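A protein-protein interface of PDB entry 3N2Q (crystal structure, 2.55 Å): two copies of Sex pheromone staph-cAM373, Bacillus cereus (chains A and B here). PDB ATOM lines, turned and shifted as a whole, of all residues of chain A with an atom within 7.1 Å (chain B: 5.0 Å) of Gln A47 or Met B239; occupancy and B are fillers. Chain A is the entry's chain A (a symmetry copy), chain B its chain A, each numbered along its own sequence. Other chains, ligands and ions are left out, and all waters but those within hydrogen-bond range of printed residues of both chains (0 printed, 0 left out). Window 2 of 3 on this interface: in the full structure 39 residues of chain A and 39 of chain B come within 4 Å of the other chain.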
ATOM      1  N   GLU A   7     -33.533  28.695   8.120  1.00  0.00           N
ATOM      2  CA  GLU A   7     -34.529  27.805   7.538  1.00  0.00           C
ATOM      3  C   GLU A   7     -35.310  27.016   8.598  1.00  0.00           C
ATOM      4  O   GLU A   7     -36.341  26.412   8.291  1.00  0.00           O
ATOM      5  CB  GLU A   7     -33.922  26.893   6.461  1.00  0.00           C
ATOM      6  CG  GLU A   7     -32.388  26.849   6.385  1.00  0.00           C
ATOM      7  CD  GLU A   7     -31.853  26.259   5.075  1.00  0.00           C
ATOM      8  OE1 GLU A   7     -32.655  25.928   4.180  1.00  0.00           O
ATOM      9  OE2 GLU A   7     -30.618  26.122   4.934  1.00  0.00           O
ATOM     10  N   GLN A   8     -34.835  27.053   9.843  1.00  0.00           N
ATOM     11  CA  GLN A   8     -35.547  26.445  10.951  1.00  0.00           C
ATOM     12  C   GLN A   8     -36.183  27.508  11.840  1.00  0.00           C
ATOM     13  O   GLN A   8     -35.488  28.187  12.608  1.00  0.00           O
ATOM     14  CB  GLN A   8     -34.610  25.569  11.781  1.00  0.00           C
ATOM     15  CG  GLN A   8     -35.250  25.001  13.042  1.00  0.00           C
ATOM     16  CD  GLN A   8     -34.266  24.222  13.897  1.00  0.00           C
ATOM     17  OE1 GLN A   8     -33.929  23.068  13.582  1.00  0.00           O
ATOM     18  NE2 GLN A   8     -33.797  24.848  14.989  1.00  0.00           N
ATOM     19  N   VAL A  45     -21.414  17.473   8.152  1.00  0.00           N
ATOM     20  CA  VAL A  45     -21.910  18.845   8.083  1.00  0.00           C
ATOM     21  C   VAL A  45     -23.384  18.869   8.446  1.00  0.00           C
ATOM     22  O   VAL A  45     -24.168  18.078   7.926  1.00  0.00           O
ATOM     23  CB  VAL A  45     -21.766  19.434   6.669  1.00  0.00           C
ATOM     24  CG1 VAL A  45     -22.120  20.894   6.677  1.00  0.00           C
ATOM     25  CG2 VAL A  45     -20.377  19.256   6.167  1.00  0.00           C
ATOM     26  N   LEU A  46     -23.748  19.792   9.331  1.00  0.00           N
ATOM     27  CA  LEU A  46     -25.123  19.910   9.813  1.00  0.00           C
ATOM     28  C   LEU A  46     -25.884  21.008   9.074  1.00  0.00           C
ATOM     29  O   LEU A  46     -25.453  22.172   9.042  1.00  0.00           O
ATOM     30  CB  LEU A  46     -25.164  20.140  11.336  1.00  0.00           C
ATOM     31  CG  LEU A  46     -26.532  20.492  11.961  1.00  0.00           C
ATOM     32  CD1 LEU A  46     -27.558  19.409  11.729  1.00  0.00           C
ATOM     33  CD2 LEU A  46     -26.453  20.829  13.453  1.00  0.00           C
ATOM     34  N   GLN A  47     -27.005  20.615   8.473  1.00  0.00           N
ATOM     35  CA  GLN A  47     -27.990  21.548   7.924  1.00  0.00           C
ATOM     36  C   GLN A  47     -29.375  21.325   8.551  1.00  0.00           C
ATOM     37  O   GLN A  47     -29.708  20.224   9.019  1.00  0.00           O
ATOM     38  CB  GLN A  47     -28.111  21.422   6.407  1.00  0.00           C
ATOM     39  CG  GLN A  47     -26.873  21.757   5.617  1.00  0.00           C
ATOM     40  CD  GLN A  47     -27.154  21.837   4.115  1.00  0.00           C
ATOM     41  OE1 GLN A  47     -27.780  22.788   3.647  1.00  0.00           O
ATOM     42  NE2 GLN A  47     -26.683  20.850   3.357  1.00  0.00           N
ATOM     43  N   LEU A  48     -30.196  22.369   8.513  1.00  0.00           N
ATOM     44  CA  LEU A  48     -31.486  22.354   9.171  1.00  0.00           C
ATOM     45  C   LEU A  48     -32.658  22.287   8.196  1.00  0.00           C
ATOM     46  O   LEU A  48     -32.677  22.984   7.167  1.00  0.00           O
ATOM     47  CB  LEU A  48     -31.624  23.582  10.066  1.00  0.00           C
ATOM     48  CG  LEU A  48     -30.536  23.848  11.114  1.00  0.00           C
ATOM     49  CD1 LEU A  48     -30.945  25.050  11.973  1.00  0.00           C
ATOM     50  CD2 LEU A  48     -30.282  22.634  11.985  1.00  0.00           C
ATOM     51  N   ASN A  49     -33.636  21.442   8.532  1.00  0.00           N
ATOM     52  CA  ASN A  49     -34.959  21.509   7.913  1.00  0.00           C
ATOM     53  C   ASN A  49     -34.949  21.338   6.394  1.00  0.00           C
ATOM     54  O   ASN A  49     -35.582  22.113   5.679  1.00  0.00           O
ATOM     55  CB  ASN A  49     -35.643  22.838   8.289  1.00  0.00           C
ATOM     56  CG  ASN A  49     -36.345  22.787   9.654  1.00  0.00           C
ATOM     57  OD1 ASN A  49     -35.813  22.256  10.656  1.00  0.00           O
ATOM     58  ND2 ASN A  49     -37.541  23.362   9.706  1.00  0.00           N
ATOM     59  N   GLN A  50     -34.245  20.325   5.902  1.00  0.00           N
ATOM     60  CA  GLN A  50     -34.077  20.182   4.455  1.00  0.00           C
ATOM     61  C   GLN A  50     -35.231  19.471   3.738  1.00  0.00           C
ATOM     62  O   GLN A  50     -35.496  19.749   2.576  1.00  0.00           O
ATOM     63  CB  GLN A  50     -32.752  19.491   4.125  1.00  0.00           C
ATOM     64  CG  GLN A  50     -31.520  20.298   4.506  1.00  0.00           C
ATOM     65  CD  GLN A  50     -31.390  21.599   3.731  1.00  0.00           C
ATOM     66  OE1 GLN A  50     -31.565  22.682   4.289  1.00  0.00           O
ATOM     67  NE2 GLN A  50     -31.081  21.500   2.445  1.00  0.00           N
ATOM     68  N   TYR A  51     -35.916  18.566   4.434  1.00  0.00           N
ATOM     69  CA  TYR A  51     -36.858  17.665   3.772  1.00  0.00           C
ATOM     70  C   TYR A  51     -38.318  17.797   4.166  1.00  0.00           C
ATOM     71  O   TYR A  51     -39.187  17.502   3.335  1.00  0.00           O
ATOM     72  CB  TYR A  51     -36.392  16.211   3.878  1.00  0.00           C
ATOM     73  CG  TYR A  51     -34.996  16.065   3.362  1.00  0.00           C
ATOM     74  CD1 TYR A  51     -34.711  16.315   2.019  1.00  0.00           C
ATOM     75  CD2 TYR A  51     -33.947  15.734   4.219  1.00  0.00           C
ATOM     76  CE1 TYR A  51     -33.430  16.219   1.538  1.00  0.00           C
ATOM     77  CE2 TYR A  51     -32.656  15.629   3.745  1.00  0.00           C
ATOM     78  CZ  TYR A  51     -32.406  15.877   2.400  1.00  0.00           C
ATOM     79  OH  TYR A  51     -31.126  15.776   1.908  1.00  0.00           O
ATOM     80  N   GLU A  74     -35.737  19.705  12.514  1.00  0.00           N
ATOM     81  CA  GLU A  74     -35.131  18.726  11.633  1.00  0.00           C
ATOM     82  C   GLU A  74     -33.658  19.032  11.489  1.00  0.00           C
ATOM     83  O   GLU A  74     -33.284  20.108  11.015  1.00  0.00           O
ATOM     84  CB  GLU A  74     -35.809  18.738  10.262  1.00  0.00           C
ATOM     85  CG  GLU A  74     -35.189  17.780   9.277  1.00  0.00           C
ATOM     86  CD  GLU A  74     -35.685  17.985   7.864  1.00  0.00           C
ATOM     87  OE1 GLU A  74     -36.680  18.734   7.680  1.00  0.00           O
ATOM     88  OE2 GLU A  74     -35.081  17.398   6.931  1.00  0.00           O
ATOM     89  N   GLN A  75     -32.829  18.082  11.898  1.00  0.00           N
ATOM     90  CA  GLN A  75     -31.395  18.213  11.738  1.00  0.00           C
ATOM     91  C   GLN A  75     -30.853  17.162  10.763  1.00  0.00           C
ATOM     92  O   GLN A  75     -30.973  15.951  10.996  1.00  0.00           O
ATOM     93  CB  GLN A  75     -30.706  18.121  13.093  1.00  0.00           C
ATOM     94  CG  GLN A  75     -30.990  19.305  14.007  1.00  0.00           C
ATOM     95  CD  GLN A  75     -30.370  19.124  15.378  1.00  0.00           C
ATOM     96  OE1 GLN A  75     -29.814  18.071  15.678  1.00  0.00           O
ATOM     97  NE2 GLN A  75     -30.468  20.145  16.221  1.00  0.00           N
ATOM     98  N   ASP A  76     -30.252  17.642   9.677  1.00  0.00           N
ATOM     99  CA  ASP A  76     -29.766  16.784   8.605  1.00  0.00           C
ATOM    100  C   ASP A  76     -28.239  16.738   8.583  1.00  0.00           C
ATOM    101  O   ASP A  76     -27.589  17.779   8.488  1.00  0.00           O
ATOM    102  CB  ASP A  76     -30.317  17.285   7.264  1.00  0.00           C
ATOM    103  CG  ASP A  76     -31.809  17.592   7.320  1.00  0.00           C
ATOM    104  OD1 ASP A  76     -32.180  18.788   7.243  1.00  0.00           O
ATOM    105  OD2 ASP A  76     -32.605  16.643   7.472  1.00  0.00           O
ATOM    106  N   TYR A  77     -27.677  15.527   8.654  1.00  0.00           N
ATOM    107  CA  TYR A  77     -26.223  15.341   8.722  1.00  0.00           C
ATOM    108  C   TYR A  77     -25.677  14.746   7.447  1.00  0.00           C
ATOM    109  O   TYR A  77     -26.131  13.691   7.003  1.00  0.00           O
ATOM    110  CB  TYR A  77     -25.850  14.446   9.904  1.00  0.00           C
ATOM    111  CG  TYR A  77     -26.182  15.063  11.234  1.00  0.00           C
ATOM    112  CD1 TYR A  77     -27.482  15.061  11.705  1.00  0.00           C
ATOM    113  CD2 TYR A  77     -25.195  15.662  12.010  1.00  0.00           C
ATOM    114  CE1 TYR A  77     -27.803  15.636  12.911  1.00  0.00           C
ATOM    115  CE2 TYR A  77     -25.495  16.244  13.223  1.00  0.00           C
ATOM    116  CZ  TYR A  77     -26.808  16.227  13.675  1.00  0.00           C
ATOM    117  OH  TYR A  77     -27.142  16.789  14.895  1.00  0.00           O
ATOM    118  N   PHE A  78     -24.684  15.422   6.877  1.00  0.00           N
ATOM    119  CA  PHE A  78     -24.059  15.010   5.621  1.00  0.00           C
ATOM    120  C   PHE A  78     -22.614  14.636   5.873  1.00  0.00           C
ATOM    121  O   PHE A  78     -21.870  15.406   6.467  1.00  0.00           O
ATOM    122  CB  PHE A  78     -24.120  16.133   4.582  1.00  0.00           C
ATOM    123  CG  PHE A  78     -25.518  16.601   4.266  1.00  0.00           C
ATOM    124  CD1 PHE A  78     -26.234  17.389   5.180  1.00  0.00           C
ATOM    125  CD2 PHE A  78     -26.116  16.269   3.049  1.00  0.00           C
ATOM    126  CE1 PHE A  78     -27.527  17.825   4.897  1.00  0.00           C
ATOM    127  CE2 PHE A  78     -27.416  16.702   2.745  1.00  0.00           C
ATOM    128  CZ  PHE A  78     -28.126  17.481   3.675  1.00  0.00           C
ATOM    129  N   LEU A  86     -19.418  14.313  -0.028  1.00  0.00           N
ATOM    130  CA  LEU A  86     -20.498  14.671   0.929  1.00  0.00           C
ATOM    131  C   LEU A  86     -21.948  14.505   0.462  1.00  0.00           C
ATOM    132  O   LEU A  86     -22.406  15.187  -0.451  1.00  0.00           O
ATOM    133  CB  LEU A  86     -20.304  16.080   1.511  1.00  0.00           C
ATOM    134  CG  LEU A  86     -19.265  16.293   2.617  1.00  0.00           C
ATOM    135  CD1 LEU A  86     -19.057  17.766   2.884  1.00  0.00           C
ATOM    136  CD2 LEU A  86     -19.675  15.631   3.894  1.00  0.00           C
ATOM    137  N   SER A  87     -22.663  13.604   1.127  1.00  0.00           N
ATOM    138  CA  SER A  87     -24.099  13.399   0.919  1.00  0.00           C
ATOM    139  C   SER A  87     -24.726  13.107   2.275  1.00  0.00           C
ATOM    140  O   SER A  87     -24.029  13.137   3.282  1.00  0.00           O
ATOM    141  CB  SER A  87     -24.352  12.233  -0.038  1.00  0.00           C
ATOM    142  OG  SER A  87     -24.187  11.006   0.647  1.00  0.00           O
ATOM    143  N   LEU A  88     -26.026  12.804   2.295  1.00  0.00           N
ATOM    144  CA  LEU A  88     -26.788  12.634   3.535  1.00  0.00           C
ATOM    145  C   LEU A  88     -26.533  11.295   4.255  1.00  0.00           C
ATOM    146  O   LEU A  88     -26.525  10.256   3.609  1.00  0.00           O
ATOM    147  CB  LEU A  88     -28.281  12.801   3.237  1.00  0.00           C
ATOM    148  CG  LEU A  88     -29.245  12.701   4.433  1.00  0.00           C
ATOM    149  CD1 LEU A  88     -28.996  13.805   5.469  1.00  0.00           C
ATOM    150  CD2 LEU A  88     -30.703  12.697   3.975  1.00  0.00           C
ATOM    151  N   LYS B 235     -21.663  23.821  -5.811  1.00  0.00           N
ATOM    152  CA  LYS B 235     -22.071  23.549  -4.430  1.00  0.00           C
ATOM    153  C   LYS B 235     -21.243  22.453  -3.771  1.00  0.00           C
ATOM    154  O   LYS B 235     -20.944  22.531  -2.572  1.00  0.00           O
ATOM    155  CB  LYS B 235     -23.560  23.196  -4.339  1.00  0.00           C
ATOM    156  CG  LYS B 235     -24.095  23.213  -2.902  1.00  0.00           C
ATOM    157  CD  LYS B 235     -25.597  22.972  -2.837  1.00  0.00           C
ATOM    158  CE  LYS B 235     -26.091  23.021  -1.390  1.00  0.00           C
ATOM    159  NZ  LYS B 235     -27.549  22.748  -1.280  1.00  0.00           N
ATOM    160  N   THR B 236     -20.891  21.432  -4.556  1.00  0.00           N
ATOM    161  CA  THR B 236     -20.046  20.341  -4.083  1.00  0.00           C
ATOM    162  C   THR B 236     -18.779  20.885  -3.414  1.00  0.00           C
ATOM    163  O   THR B 236     -18.482  20.536  -2.272  1.00  0.00           O
ATOM    164  CB  THR B 236     -19.656  19.392  -5.220  1.00  0.00           C
ATOM    165  OG1 THR B 236     -18.936  20.130  -6.213  1.00  0.00           O
ATOM    166  CG2 THR B 236     -20.902  18.744  -5.848  1.00  0.00           C
ATOM    167  N   GLU B 237     -18.054  21.755  -4.119  1.00  0.00           N
ATOM    168  CA  GLU B 237     -16.831  22.351  -3.576  1.00  0.00           C
ATOM    169  C   GLU B 237     -17.129  23.147  -2.307  1.00  0.00           C
ATOM    170  O   GLU B 237     -16.453  22.996  -1.297  1.00  0.00           O
ATOM    171  CB  GLU B 237     -16.148  23.241  -4.619  1.00  0.00           C
ATOM    172  CG  GLU B 237     -15.698  22.506  -5.877  1.00  0.00           C
ATOM    173  CD  GLU B 237     -14.385  21.745  -5.706  1.00  0.00           C
ATOM    174  OE1 GLU B 237     -13.592  22.088  -4.799  1.00  0.00           O
ATOM    175  OE2 GLU B 237     -14.142  20.802  -6.492  1.00  0.00           O
ATOM    176  N   LEU B 238     -18.163  23.977  -2.361  1.00  0.00           N
ATOM    177  CA  LEU B 238     -18.555  24.800  -1.228  1.00  0.00           C
ATOM    178  C   LEU B 238     -18.985  23.973  -0.001  1.00  0.00           C
ATOM    179  O   LEU B 238     -18.822  24.407   1.145  1.00  0.00           O
ATOM    180  CB  LEU B 238     -19.672  25.758  -1.655  1.00  0.00           C
ATOM    181  CG  LEU B 238     -20.220  26.763  -0.637  1.00  0.00           C
ATOM    182  CD1 LEU B 238     -19.168  27.812  -0.364  1.00  0.00           C
ATOM    183  CD2 LEU B 238     -21.498  27.414  -1.137  1.00  0.00           C
ATOM    184  N   MET B 239     -19.537  22.787  -0.236  1.00  0.00           N
ATOM    185  CA  MET B 239     -19.870  21.881   0.864  1.00  0.00           C
ATOM    186  C   MET B 239     -18.612  21.413   1.617  1.00  0.00           C
ATOM    187  O   MET B 239     -18.508  21.588   2.841  1.00  0.00           O
ATOM    188  CB  MET B 239     -20.647  20.681   0.348  1.00  0.00           C
ATOM    189  CG  MET B 239     -21.243  19.851   1.454  1.00  0.00           C
ATOM    190  SD  MET B 239     -22.949  20.555   2.041  1.00  0.00           S
ATOM    191  CE  MET B 239     -24.117  19.369   0.998  1.00  0.00           C
ATOM    192  N   ALA B 240     -17.664  20.833   0.869  1.00  0.00           N
ATOM    193  CA  ALA B 240     -16.378  20.378   1.407  1.00  0.00           C
ATOM    194  C   ALA B 240     -15.699  21.469   2.238  1.00  0.00           C
ATOM    195  O   ALA B 240     -15.150  21.202   3.307  1.00  0.00           O
ATOM    196  CB  ALA B 240     -15.455  19.904   0.271  1.00  0.00           C
ATOM    197  N   LEU B 241     -15.762  22.697   1.739  1.00  0.00           N
ATOM    198  CA  LEU B 241     -15.214  23.860   2.439  1.00  0.00           C
ATOM    199  C   LEU B 241     -15.973  24.176   3.723  1.00  0.00           C
ATOM    200  O   LEU B 241     -15.353  24.518   4.719  1.00  0.00           O
ATOM    201  CB  LEU B 241     -15.180  25.088   1.522  1.00  0.00           C
ATOM    202  CG  LEU B 241     -14.724  26.420   2.124  1.00  0.00           C
ATOM    203  CD1 LEU B 241     -13.353  26.323   2.797  1.00  0.00           C
ATOM    204  CD2 LEU B 241     -14.701  27.496   1.050  1.00  0.00           C
ATOM    205  N   THR B 242     -17.303  24.057   3.709  1.00  0.00           N
ATOM    206  CA  THR B 242     -18.079  24.307   4.931  1.00  0.00           C
ATOM    207  C   THR B 242     -17.779  23.258   5.994  1.00  0.00           C
ATOM    208  O   THR B 242     -17.797  23.576   7.176  1.00  0.00           O
ATOM    209  CB  THR B 242     -19.602  24.381   4.706  1.00  0.00           C
ATOM    210  OG1 THR B 242     -20.032  23.214   4.012  1.00  0.00           O
ATOM    211  CG2 THR B 242     -19.968  25.586   3.889  1.00  0.00           C
ATOM    212  N   GLN B 243     -17.476  22.025   5.578  1.00  0.00           N
ATOM    213  CA  GLN B 243     -17.118  20.984   6.544  1.00  0.00           C
ATOM    214  C   GLN B 243     -15.733  21.201   7.136  1.00  0.00           C
ATOM    215  O   GLN B 243     -15.529  21.011   8.334  1.00  0.00           O
ATOM    216  CB  GLN B 243     -17.300  19.563   5.981  1.00  0.00           C
ATOM    217  CG  GLN B 243     -16.049  18.797   5.634  1.00  0.00           C
ATOM    218  CD  GLN B 243     -16.167  17.338   6.003  1.00  0.00           C
ATOM    219  OE1 GLN B 243     -16.116  16.989   7.180  1.00  0.00           O
ATOM    220  NE2 GLN B 243     -16.320  16.473   5.003  1.00  0.00           N
ATOM    221  N   VAL B 284     -24.950  24.897   8.940  1.00  0.00           N
ATOM    222  CA  VAL B 284     -24.695  25.616   7.693  1.00  0.00           C
ATOM    223  C   VAL B 284     -26.001  25.940   6.989  1.00  0.00           C
ATOM    224  O   VAL B 284     -26.894  25.085   6.907  1.00  0.00           O
ATOM    225  CB  VAL B 284     -23.809  24.782   6.745  1.00  0.00           C
ATOM    226  CG1 VAL B 284     -23.421  25.571   5.512  1.00  0.00           C
ATOM    227  CG2 VAL B 284     -22.577  24.300   7.468  1.00  0.00           C
ATOM    228  N   PHE B 286     -27.311  27.650   3.238  1.00  0.00           N
ATOM    229  CA  PHE B 286     -26.928  28.072   1.907  1.00  0.00           C
ATOM    230  C   PHE B 286     -27.922  29.081   1.378  1.00  0.00           C
ATOM    231  O   PHE B 286     -29.094  29.057   1.745  1.00  0.00           O
ATOM    232  CB  PHE B 286     -26.789  26.864   0.976  1.00  0.00           C
ATOM    233  CG  PHE B 286     -25.660  25.945   1.355  1.00  0.00           C
ATOM    234  CD1 PHE B 286     -24.361  26.192   0.912  1.00  0.00           C
ATOM    235  CD2 PHE B 286     -25.883  24.845   2.171  1.00  0.00           C
ATOM    236  CE1 PHE B 286     -23.294  25.344   1.270  1.00  0.00           C
ATOM    237  CE2 PHE B 286     -24.821  23.990   2.535  1.00  0.00           C
ATOM    238  CZ  PHE B 286     -23.523  24.248   2.084  1.00  0.00           C
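Hydrophobic or aromatic side chains of chain A within 4 Å of the printed part of chain B: Val A45 and Leu A86. Among the printed residues, 9 pairs touch across the chains.
Of the printed residues of chain B, Val A45 touches Gln B243 (3.1 Å) and Val B284 (3.5 Å). Printed residues of chain B within 4 Å of Gln A47: Met B239 (3.8 Å), Val B284 (3.6 Å) and Phe B286 (3.2 Å). Printed residues of chain B within 4 Å of Leu A86: Met B239 (3.3 Å), Ala B240 (3.9 Å) and Gln B243 (3.6 Å). Ser A87 touches none of the printed residues of chain B. Met B239 touches two residues of chain A. Printed residues of chain A within 4 Å of Gln B243: Val A45 (3.1 Å) and Leu A86 (3.6 Å). Of the printed residues of chain A, Val B284 touches Val A45, Leu A46 and Gln A47. The nearest residue of chain B that does not touch Gln A47 is Lys B235 (4.9 Å). The nearest printed residue of chain B that does not touch Val A45 is Thr B242 (4.1 Å).
Gln B243 touches Val A45 (CB to CG2, 3.1 Å). Val B284 touches Val A45 (CG2 to CG1, 3.5 Å). Gln A47 touches Met B239. CG of Gln A47 touches O of Val B284 (3.6 Å). Phe B286 touches Gln A47 (CD2 to OE1, 3.2 Å). Leu A86 touches Met B239. Leu A86 touches Ala B240. NE2 of Gln B243 touches CD2 of Leu A86 (3.6 Å).
The backbone NH (N) of Asp A76 is in hydrogen-bond range of the backbone carbonyl oxygen (O) of Gln A47 (2.7 Å). The backbone carbonyl oxygen (O) of Met B239 is in hydrogen-bond range of the side-chain hydroxyl (OG1) of Thr B242 (2.5 Å). The backbone carbonyl oxygen (O) of Phe A78 sits at hydrogen-bond distance from the backbone NH (N) of Val A45, 2.7 Å away.
No position is printed for both chains.
O of Leu A46 sits at hydrogen-bond distance from N of Val B284 (2.8 Å).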
